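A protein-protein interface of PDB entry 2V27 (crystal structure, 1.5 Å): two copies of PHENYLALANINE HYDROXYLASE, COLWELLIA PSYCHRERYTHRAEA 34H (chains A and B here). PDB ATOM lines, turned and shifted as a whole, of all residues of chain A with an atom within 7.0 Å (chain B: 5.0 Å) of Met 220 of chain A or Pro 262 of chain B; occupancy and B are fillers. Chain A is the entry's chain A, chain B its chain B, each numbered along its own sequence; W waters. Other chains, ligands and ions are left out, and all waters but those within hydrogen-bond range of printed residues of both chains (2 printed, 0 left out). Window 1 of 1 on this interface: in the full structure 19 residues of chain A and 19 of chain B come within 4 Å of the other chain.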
ATOM      1  N   GLY A 189      20.067 -10.928  23.444  1.00  0.00           N
ATOM      2  CA  GLY A 189      21.193  -9.980  23.656  1.00  0.00           C
ATOM      3  C   GLY A 189      22.440 -10.752  24.029  1.00  0.00           C
ATOM      4  O   GLY A 189      23.538 -10.490  23.506  1.00  0.00           O
ATOM      5  N   GLU A 190      22.304 -11.717  24.933  1.00  0.00           N
ATOM      6  CA  GLU A 190      23.496 -12.478  25.358  1.00  0.00           C
ATOM      7  C   GLU A 190      24.003 -13.379  24.222  1.00  0.00           C
ATOM      8  O   GLU A 190      25.220 -13.554  24.095  1.00  0.00           O
ATOM      9  CB  GLU A 190      23.205 -13.357  26.586  1.00  0.00           C
ATOM     10  CG  GLU A 190      22.803 -12.573  27.824  1.00  0.00           C
ATOM     11  CD  GLU A 190      23.902 -11.670  28.389  1.00  0.00           C
ATOM     12  OE1 GLU A 190      25.070 -11.800  27.966  1.00  0.00           O
ATOM     13  OE2 GLU A 190      23.582 -10.829  29.311  1.00  0.00           O
ATOM     14  N   ASP A 192      23.737 -12.968  20.913  1.00  0.00           N
ATOM     15  CA  ASP A 192      24.444 -12.226  19.861  1.00  0.00           C
ATOM     16  C   ASP A 192      25.829 -11.776  20.300  1.00  0.00           C
ATOM     17  O   ASP A 192      26.783 -11.880  19.560  1.00  0.00           O
ATOM     18  CB  ASP A 192      23.654 -11.003  19.372  1.00  0.00           C
ATOM     19  CG  ASP A 192      24.305 -10.371  18.150  1.00  0.00           C
ATOM     20  OD1 ASP A 192      24.934  -9.335  18.270  1.00  0.00           O
ATOM     21  OD2 ASP A 192      24.260 -11.001  17.092  1.00  0.00           O
ATOM     22  N   TYR A 193      25.952 -11.319  21.523  1.00  0.00           N
ATOM     23  CA  TYR A 193      27.223 -10.837  22.004  1.00  0.00           C
ATOM     24  C   TYR A 193      28.218 -12.004  22.157  1.00  0.00           C
ATOM     25  O   TYR A 193      29.361 -11.900  21.713  1.00  0.00           O
ATOM     26  CB  TYR A 193      26.993 -10.064  23.292  1.00  0.00           C
ATOM     27  CG  TYR A 193      28.249  -9.558  23.953  1.00  0.00           C
ATOM     28  CD1 TYR A 193      28.806  -8.288  23.634  1.00  0.00           C
ATOM     29  CD2 TYR A 193      28.858 -10.337  24.959  1.00  0.00           C
ATOM     30  CE1 TYR A 193      30.002  -7.845  24.314  1.00  0.00           C
ATOM     31  CE2 TYR A 193      29.986  -9.936  25.593  1.00  0.00           C
ATOM     32  CZ  TYR A 193      30.535  -8.709  25.312  1.00  0.00           C
ATOM     33  OH  TYR A 193      31.689  -8.410  26.055  1.00  0.00           O
ATOM     34  N   ALA A 194      27.817 -13.096  22.809  1.00  0.00           N
ATOM     35  CA  ALA A 194      28.736 -14.218  23.020  1.00  0.00           C
ATOM     36  C   ALA A 194      29.253 -14.777  21.682  1.00  0.00           C
ATOM     37  O   ALA A 194      30.417 -15.159  21.575  1.00  0.00           O
ATOM     38  CB  ALA A 194      28.069 -15.337  23.876  1.00  0.00           C
ATOM     39  N   VAL A 200      35.756  -9.455  22.527  1.00  0.00           N
ATOM     40  CA  VAL A 200      35.670 -10.184  23.771  1.00  0.00           C
ATOM     41  C   VAL A 200      36.654 -11.374  23.789  1.00  0.00           C
ATOM     42  O   VAL A 200      36.930 -11.944  22.749  1.00  0.00           O
ATOM     43  CB  VAL A 200      34.222 -10.620  23.988  1.00  0.00           C
ATOM     44  CG1 VAL A 200      33.744 -11.692  22.914  1.00  0.00           C
ATOM     45  CG2 VAL A 200      34.031 -11.047  25.389  1.00  0.00           C
ATOM     46  N   ARG A 216      31.330  -9.616  36.949  1.00  0.00           N
ATOM     47  CA  ARG A 216      30.235  -8.775  37.412  1.00  0.00           C
ATOM     48  C   ARG A 216      28.990  -9.193  36.683  1.00  0.00           C
ATOM     49  O   ARG A 216      29.044  -9.460  35.478  1.00  0.00           O
ATOM     50  CB  ARG A 216      30.530  -7.290  37.201  1.00  0.00           C
ATOM     51  CG  ARG A 216      31.796  -6.845  37.942  1.00  0.00           C
ATOM     52  CD  ARG A 216      31.586  -6.675  39.427  1.00  0.00           C
ATOM     53  NE  ARG A 216      32.823  -6.266  40.125  1.00  0.00           N
ATOM     54  CZ  ARG A 216      33.700  -7.087  40.714  1.00  0.00           C
ATOM     55  NH1 ARG A 216      33.535  -8.403  40.690  1.00  0.00           N
ATOM     56  NH2 ARG A 216      34.755  -6.563  41.351  1.00  0.00           N
ATOM     57  N   ILE A 217      27.854  -9.192  37.368  1.00  0.00           N
ATOM     58  CA  ILE A 217      26.686  -9.763  36.746  1.00  0.00           C
ATOM     59  C   ILE A 217      25.933  -8.830  35.809  1.00  0.00           C
ATOM     60  O   ILE A 217      25.127  -9.305  35.002  1.00  0.00           O
ATOM     61  CB  ILE A 217      25.696 -10.348  37.763  1.00  0.00           C
ATOM     62  CG1 ILE A 217      25.118  -9.265  38.654  1.00  0.00           C
ATOM     63  CG2 ILE A 217      26.427 -11.407  38.684  1.00  0.00           C
ATOM     64  CD1 ILE A 217      24.019  -9.774  39.677  1.00  0.00           C
ATOM     65  N   ASP A 218      26.155  -7.530  35.969  1.00  0.00           N
ATOM     66  CA  ASP A 218      25.351  -6.569  35.210  1.00  0.00           C
ATOM     67  C   ASP A 218      26.097  -5.866  34.090  1.00  0.00           C
ATOM     68  O   ASP A 218      25.691  -4.787  33.633  1.00  0.00           O
ATOM     69  CB  ASP A 218      24.689  -5.563  36.140  1.00  0.00           C
ATOM     70  CG  ASP A 218      25.677  -4.865  37.038  1.00  0.00           C
ATOM     71  OD1 ASP A 218      26.906  -5.121  36.965  1.00  0.00           O
ATOM     72  OD2 ASP A 218      25.238  -4.037  37.880  1.00  0.00           O
ATOM     73  N   ILE A 219      27.170  -6.508  33.649  1.00  0.00           N
ATOM     74  CA  ILE A 219      27.928  -5.973  32.511  1.00  0.00           C
ATOM     75  C   ILE A 219      27.977  -6.989  31.389  1.00  0.00           C
ATOM     76  O   ILE A 219      27.694  -8.178  31.619  1.00  0.00           O
ATOM     77  CB  ILE A 219      29.401  -5.528  32.868  1.00  0.00           C
ATOM     78  CG1 ILE A 219      30.233  -6.746  33.318  1.00  0.00           C
ATOM     79  CG2 ILE A 219      29.354  -4.453  33.996  1.00  0.00           C
ATOM     80  CD1 ILE A 219      31.743  -6.427  33.428  1.00  0.00           C
ATOM     81  N   MET A 220      28.293  -6.530  30.169  1.00  0.00           N
ATOM     82  CA  MET A 220      28.631  -7.486  29.093  1.00  0.00           C
ATOM     83  C   MET A 220      29.958  -8.176  29.415  1.00  0.00           C
ATOM     84  O   MET A 220      30.944  -7.524  29.788  1.00  0.00           O
ATOM     85  CB  MET A 220      28.695  -6.753  27.788  1.00  0.00           C
ATOM     86  CG  MET A 220      27.446  -5.924  27.427  1.00  0.00           C
ATOM     87  SD  MET A 220      25.909  -6.931  27.530  1.00  0.00           S
ATOM     88  CE  MET A 220      26.121  -8.104  26.162  1.00  0.00           C
ATOM     89  N   GLN A 221      29.924  -9.492  29.407  1.00  0.00           N
ATOM     90  CA  GLN A 221      31.038 -10.240  29.939  1.00  0.00           C
ATOM     91  C   GLN A 221      32.313 -10.079  29.099  1.00  0.00           C
ATOM     92  O   GLN A 221      32.285 -10.315  27.888  1.00  0.00           O
ATOM     93  CB  GLN A 221      30.598 -11.724  29.988  1.00  0.00           C
ATOM     94  CG  GLN A 221      29.477 -12.050  31.017  1.00  0.00           C
ATOM     95  CD  GLN A 221      29.855 -11.542  32.353  1.00  0.00           C
ATOM     96  OE1 GLN A 221      30.784 -12.055  32.978  1.00  0.00           O
ATOM     97  NE2 GLN A 221      29.146 -10.525  32.814  1.00  0.00           N
ATOM     98  N   PRO A 222      33.427  -9.676  29.722  1.00  0.00           N
ATOM     99  CA  PRO A 222      34.637  -9.504  28.880  1.00  0.00           C
ATOM    100  C   PRO A 222      35.448 -10.772  28.627  1.00  0.00           C
ATOM    101  O   PRO A 222      36.345 -10.784  27.730  1.00  0.00           O
ATOM    102  CB  PRO A 222      35.440  -8.480  29.668  1.00  0.00           C
ATOM    103  CG  PRO A 222      35.067  -8.752  31.180  1.00  0.00           C
ATOM    104  CD  PRO A 222      33.585  -9.135  31.102  1.00  0.00           C
ATOM    105  N   ILE A 223      35.067 -11.840  29.342  1.00  0.00           N
ATOM    106  CA  ILE A 223      35.730 -13.146  29.190  1.00  0.00           C
ATOM    107  C   ILE A 223      34.740 -14.293  29.212  1.00  0.00           C
ATOM    108  O   ILE A 223      33.850 -14.306  30.054  1.00  0.00           O
ATOM    109  CB  ILE A 223      36.744 -13.421  30.350  1.00  0.00           C
ATOM    110  CG1 ILE A 223      37.876 -12.407  30.341  1.00  0.00           C
ATOM    111  CG2 ILE A 223      37.298 -14.850  30.248  1.00  0.00           C
ATOM    112  CD1 ILE A 223      38.674 -12.413  31.670  1.00  0.00           C
ATOM    113  N   TYR A 224      34.899 -15.229  28.278  1.00  0.00           N
ATOM    114  CA  TYR A 224      34.180 -16.502  28.322  1.00  0.00           C
ATOM    115  C   TYR A 224      35.196 -17.621  28.300  1.00  0.00           C
ATOM    116  O   TYR A 224      36.269 -17.481  27.697  1.00  0.00           O
ATOM    117  CB  TYR A 224      33.285 -16.713  27.117  1.00  0.00           C
ATOM    118  CG  TYR A 224      32.124 -15.731  26.994  1.00  0.00           C
ATOM    119  CD1 TYR A 224      32.349 -14.400  26.606  1.00  0.00           C
ATOM    120  CD2 TYR A 224      30.817 -16.122  27.330  1.00  0.00           C
ATOM    121  CE1 TYR A 224      31.300 -13.477  26.540  1.00  0.00           C
ATOM    122  CE2 TYR A 224      29.754 -15.200  27.262  1.00  0.00           C
ATOM    123  CZ  TYR A 224      30.010 -13.895  26.868  1.00  0.00           C
ATOM    124  OH  TYR A 224      29.005 -12.965  26.773  1.00  0.00           O
ATOM    125  N   PRO A 262      36.448  -3.533  32.211  1.00  0.00           N
ATOM    126  CA  PRO A 262      35.001  -3.398  32.531  1.00  0.00           C
ATOM    127  C   PRO A 262      34.632  -3.898  33.887  1.00  0.00           C
ATOM    128  O   PRO A 262      33.711  -3.366  34.520  1.00  0.00           O
ATOM    129  CB  PRO A 262      34.285  -4.228  31.438  1.00  0.00           C
ATOM    130  CG  PRO A 262      35.290  -4.270  30.299  1.00  0.00           C
ATOM    131  CD  PRO A 262      36.649  -4.314  30.976  1.00  0.00           C
ATOM    132  N   VAL A 263      35.367  -4.897  34.370  1.00  0.00           N
ATOM    133  CA  VAL A 263      35.126  -5.364  35.736  1.00  0.00           C
ATOM    134  C   VAL A 263      35.547  -4.341  36.783  1.00  0.00           C
ATOM    135  O   VAL A 263      34.829  -4.087  37.751  1.00  0.00           O
ATOM    136  CB  VAL A 263      35.777  -6.741  35.979  1.00  0.00           C
ATOM    137  CG1 VAL A 263      35.741  -7.119  37.453  1.00  0.00           C
ATOM    138  CG2 VAL A 263      34.989  -7.814  35.138  1.00  0.00           C
ATOM    139  N   ILE B 219      29.305   1.317  32.858  1.00  0.00           N
ATOM    140  CA  ILE B 219      29.467   0.319  31.775  1.00  0.00           C
ATOM    141  C   ILE B 219      30.365   0.844  30.629  1.00  0.00           C
ATOM    142  O   ILE B 219      30.602   2.059  30.528  1.00  0.00           O
ATOM    143  CB  ILE B 219      28.124  -0.201  31.147  1.00  0.00           C
ATOM    144  CG1 ILE B 219      27.422   0.966  30.411  1.00  0.00           C
ATOM    145  CG2 ILE B 219      27.226  -0.796  32.217  1.00  0.00           C
ATOM    146  CD1 ILE B 219      26.182   0.489  29.639  1.00  0.00           C
ATOM    147  N   PRO B 222      28.107   1.949  24.905  1.00  0.00           N
ATOM    148  CA  PRO B 222      27.712   1.379  23.615  1.00  0.00           C
ATOM    149  C   PRO B 222      27.633   2.387  22.481  1.00  0.00           C
ATOM    150  O   PRO B 222      27.695   1.991  21.296  1.00  0.00           O
ATOM    151  CB  PRO B 222      26.333   0.745  23.893  1.00  0.00           C
ATOM    152  CG  PRO B 222      25.830   1.412  25.132  1.00  0.00           C
ATOM    153  CD  PRO B 222      27.002   1.997  25.891  1.00  0.00           C
ATOM    154  N   LYS B 260      20.214   0.533  24.330  1.00  0.00           N
ATOM    155  CA  LYS B 260      20.975  -0.606  23.863  1.00  0.00           C
ATOM    156  C   LYS B 260      20.955  -1.692  24.934  1.00  0.00           C
ATOM    157  O   LYS B 260      20.768  -1.401  26.098  1.00  0.00           O
ATOM    158  CB  LYS B 260      22.393  -0.227  23.496  1.00  0.00           C
ATOM    159  CG  LYS B 260      22.486   0.909  22.491  1.00  0.00           C
ATOM    160  CD  LYS B 260      22.258   0.350  21.122  1.00  0.00           C
ATOM    161  CE  LYS B 260      23.085   1.163  20.097  1.00  0.00           C
ATOM    162  NZ  LYS B 260      23.414   0.401  18.848  1.00  0.00           N
ATOM    163  N   PHE B 261      21.109  -2.948  24.510  1.00  0.00           N
ATOM    164  CA  PHE B 261      21.038  -4.048  25.474  1.00  0.00           C
ATOM    165  C   PHE B 261      21.928  -3.842  26.733  1.00  0.00           C
ATOM    166  O   PHE B 261      21.450  -4.110  27.840  1.00  0.00           O
ATOM    167  CB  PHE B 261      21.377  -5.363  24.757  1.00  0.00           C
ATOM    168  CG  PHE B 261      21.282  -6.556  25.639  1.00  0.00           C
ATOM    169  CD1 PHE B 261      20.022  -7.063  25.997  1.00  0.00           C
ATOM    170  CD2 PHE B 261      22.418  -7.188  26.140  1.00  0.00           C
ATOM    171  CE1 PHE B 261      19.948  -8.213  26.840  1.00  0.00           C
ATOM    172  CE2 PHE B 261      22.331  -8.301  26.966  1.00  0.00           C
ATOM    173  CZ  PHE B 261      21.093  -8.826  27.313  1.00  0.00           C
ATOM    174  N   PRO B 262      23.203  -3.367  26.591  1.00  0.00           N
ATOM    175  CA  PRO B 262      24.013  -3.160  27.820  1.00  0.00           C
ATOM    176  C   PRO B 262      23.397  -2.176  28.785  1.00  0.00           C
ATOM    177  O   PRO B 262      23.556  -2.329  29.991  1.00  0.00           O
ATOM    178  CB  PRO B 262      25.371  -2.649  27.270  1.00  0.00           C
ATOM    179  CG  PRO B 262      25.456  -3.238  25.846  1.00  0.00           C
ATOM    180  CD  PRO B 262      23.990  -3.107  25.366  1.00  0.00           C
ATOM    181  N   VAL B 263      22.692  -1.173  28.259  1.00  0.00           N
ATOM    182  CA  VAL B 263      21.963  -0.226  29.151  1.00  0.00           C
ATOM    183  C   VAL B 263      20.757  -0.884  29.847  1.00  0.00           C
ATOM    184  O   VAL B 263      20.526  -0.653  31.048  1.00  0.00           O
ATOM    185  CB  VAL B 263      21.581   1.036  28.354  1.00  0.00           C
ATOM    186  CG1 VAL B 263      20.620   1.949  29.178  1.00  0.00           C
ATOM    187  CG2 VAL B 263      22.872   1.800  27.993  1.00  0.00           C
ATOM    188  N   LYS B 264      20.052  -1.732  29.132  1.00  0.00           N
ATOM    189  CA  LYS B 264      18.956  -2.473  29.734  1.00  0.00           C
ATOM    190  C   LYS B 264      19.455  -3.343  30.888  1.00  0.00           C
ATOM    191  O   LYS B 264      18.820  -3.453  31.931  1.00  0.00           O
ATOM    192  CB  LYS B 264      18.217  -3.333  28.712  1.00  0.00           C
ATOM    193  CG  LYS B 264      17.597  -2.525  27.620  1.00  0.00           C
ATOM    194  CD  LYS B 264      16.706  -3.422  26.716  1.00  0.00           C
ATOM    195  CE  LYS B 264      16.217  -2.593  25.499  1.00  0.00           C
ATOM    196  NZ  LYS B 264      15.648  -3.453  24.400  1.00  0.00           N
ATOM    197  N   LYS B 265      20.630  -3.952  30.704  1.00  0.00           N
ATOM    198  CA  LYS B 265      21.219  -4.876  31.669  1.00  0.00           C
ATOM    199  C   LYS B 265      21.828  -4.178  32.857  1.00  0.00           C
ATOM    200  O   LYS B 265      21.813  -4.705  33.985  1.00  0.00           O
ATOM    201  CB  LYS B 265      22.252  -5.744  30.921  1.00  0.00           C
ATOM    202  CG  LYS B 265      23.012  -6.746  31.784  1.00  0.00           C
ATOM    203  CD  LYS B 265      23.851  -7.628  30.828  1.00  0.00           C
ATOM    204  CE  LYS B 265      24.529  -8.702  31.633  1.00  0.00           C
ATOM    205  NZ  LYS B 265      25.294  -9.550  30.673  1.00  0.00           N
ATOM    206  N   ALA B 266      22.305  -2.940  32.670  1.00  0.00           N
ATOM    207  CA  ALA B 266      23.019  -2.233  33.739  1.00  0.00           C
ATOM    208  C   ALA B 266      22.110  -1.922  34.922  1.00  0.00           C
ATOM    209  O   ALA B 266      20.892  -1.749  34.765  1.00  0.00           O
ATOM    210  CB  ALA B 266      23.655  -0.933  33.249  1.00  0.00           C
HETATM  211  O   HOH W   1      25.642  -3.801  31.021  1.00  0.00           O
HETATM  212  O   HOH W   2      25.845 -11.174  32.714  1.00  0.00           O
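Of chain B, only Phe 261 (3.8 Å), Pro 262 (3.7 Å) and Lys 265 (3.9 Å) come within 4 Å of Met 220 of chain A.
Of the printed residues of chain A, Pro 262 of chain B touches Met 220 (3.7 Å).
Of the printed residues of chain A, Lys 265 of chain B touches Glu 190 (2.5 Å), Ile 217 (3.5 Å), Asp 218 (3.7 Å), Ile 219 (2.9 Å) and Met 220 (3.9 Å).
Printed residues of chain B within 4 Å of Ile 217 of chain A: Lys 265 (3.5 Å).
Tyr 193 of chain A touches none of the printed residues of chain B.
The nearest printed residue of chain B that does not touch Met 220 of chain A is Ile 219 of chain B (6.2 Å).
The nearest residue of chain A that does not touch Pro 262 of chain B is Asp 218 of chain A (4.9 Å).
4 positions are printed for both chains.
The backbone carbonyl oxygen (O) of Ile 219 of chain A lies within hydrogen-bond range of the side-chain amino group (NZ) of Lys 265 of chain B, at 2.9 Å.
OE2 of Glu 190 of chain A is in salt-bridge range of NZ of Lys 265 of chain B (2.5 Å).
Printed residues of chain B that touch a printed residue of chain A: Phe 261, Pro 262, Lys 265 and Ala 266.
Printed residues of chain A that touch a printed residue of chain B: Gly 189, Glu 190, Ile 217, Asp 218, Ile 219 and Met 220.
Among the printed residues, 10 pairs touch across the chains.
Among the printed residues, Asp or Glu carboxylates within 4 Å of a Lys or Arg side-chain nitrogen of the other chain: Glu 190 of chain A with Lys 265 of chain B.
O of Ile 219 of chain A is in hydrogen-bond range of NE2 of Gln 221 of chain A (3.0 Å).
C of Gly 189 of chain A touches CE2 of Phe 261 of chain B (3.8 Å).
Glu 190 of chain A touches Phe 261 of chain B.
Ile 217 of chain A touches Lys 265 of chain B.
CB of Asp 218 of chain A touches O of Lys 265 of chain B, 3.7 Å away.
Asp 218 of chain A touches Ala 266 of chain B.
CD2 of Phe 261 of chain B touches SD of Met 220 of chain A (3.8 Å).
CG of Met 220 of chain A touches CG of Pro 262 of chain B, at 3.7 Å.
CD of Lys 265 of chain B touches SD of Met 220 of chain A (3.9 Å).
Water W2 lies within hydrogen-bond range of NZ of Lys 265 of chain B (2.7 Å), O of Ile 217 of chain A (3.0 Å) and NE2 of Gln 221 of chain A (3.4 Å).
Water W1 lies within hydrogen-bond range of O of Pro 262 of chain B (2.8 Å) and O of Asp 218 of chain A (2.8 Å).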
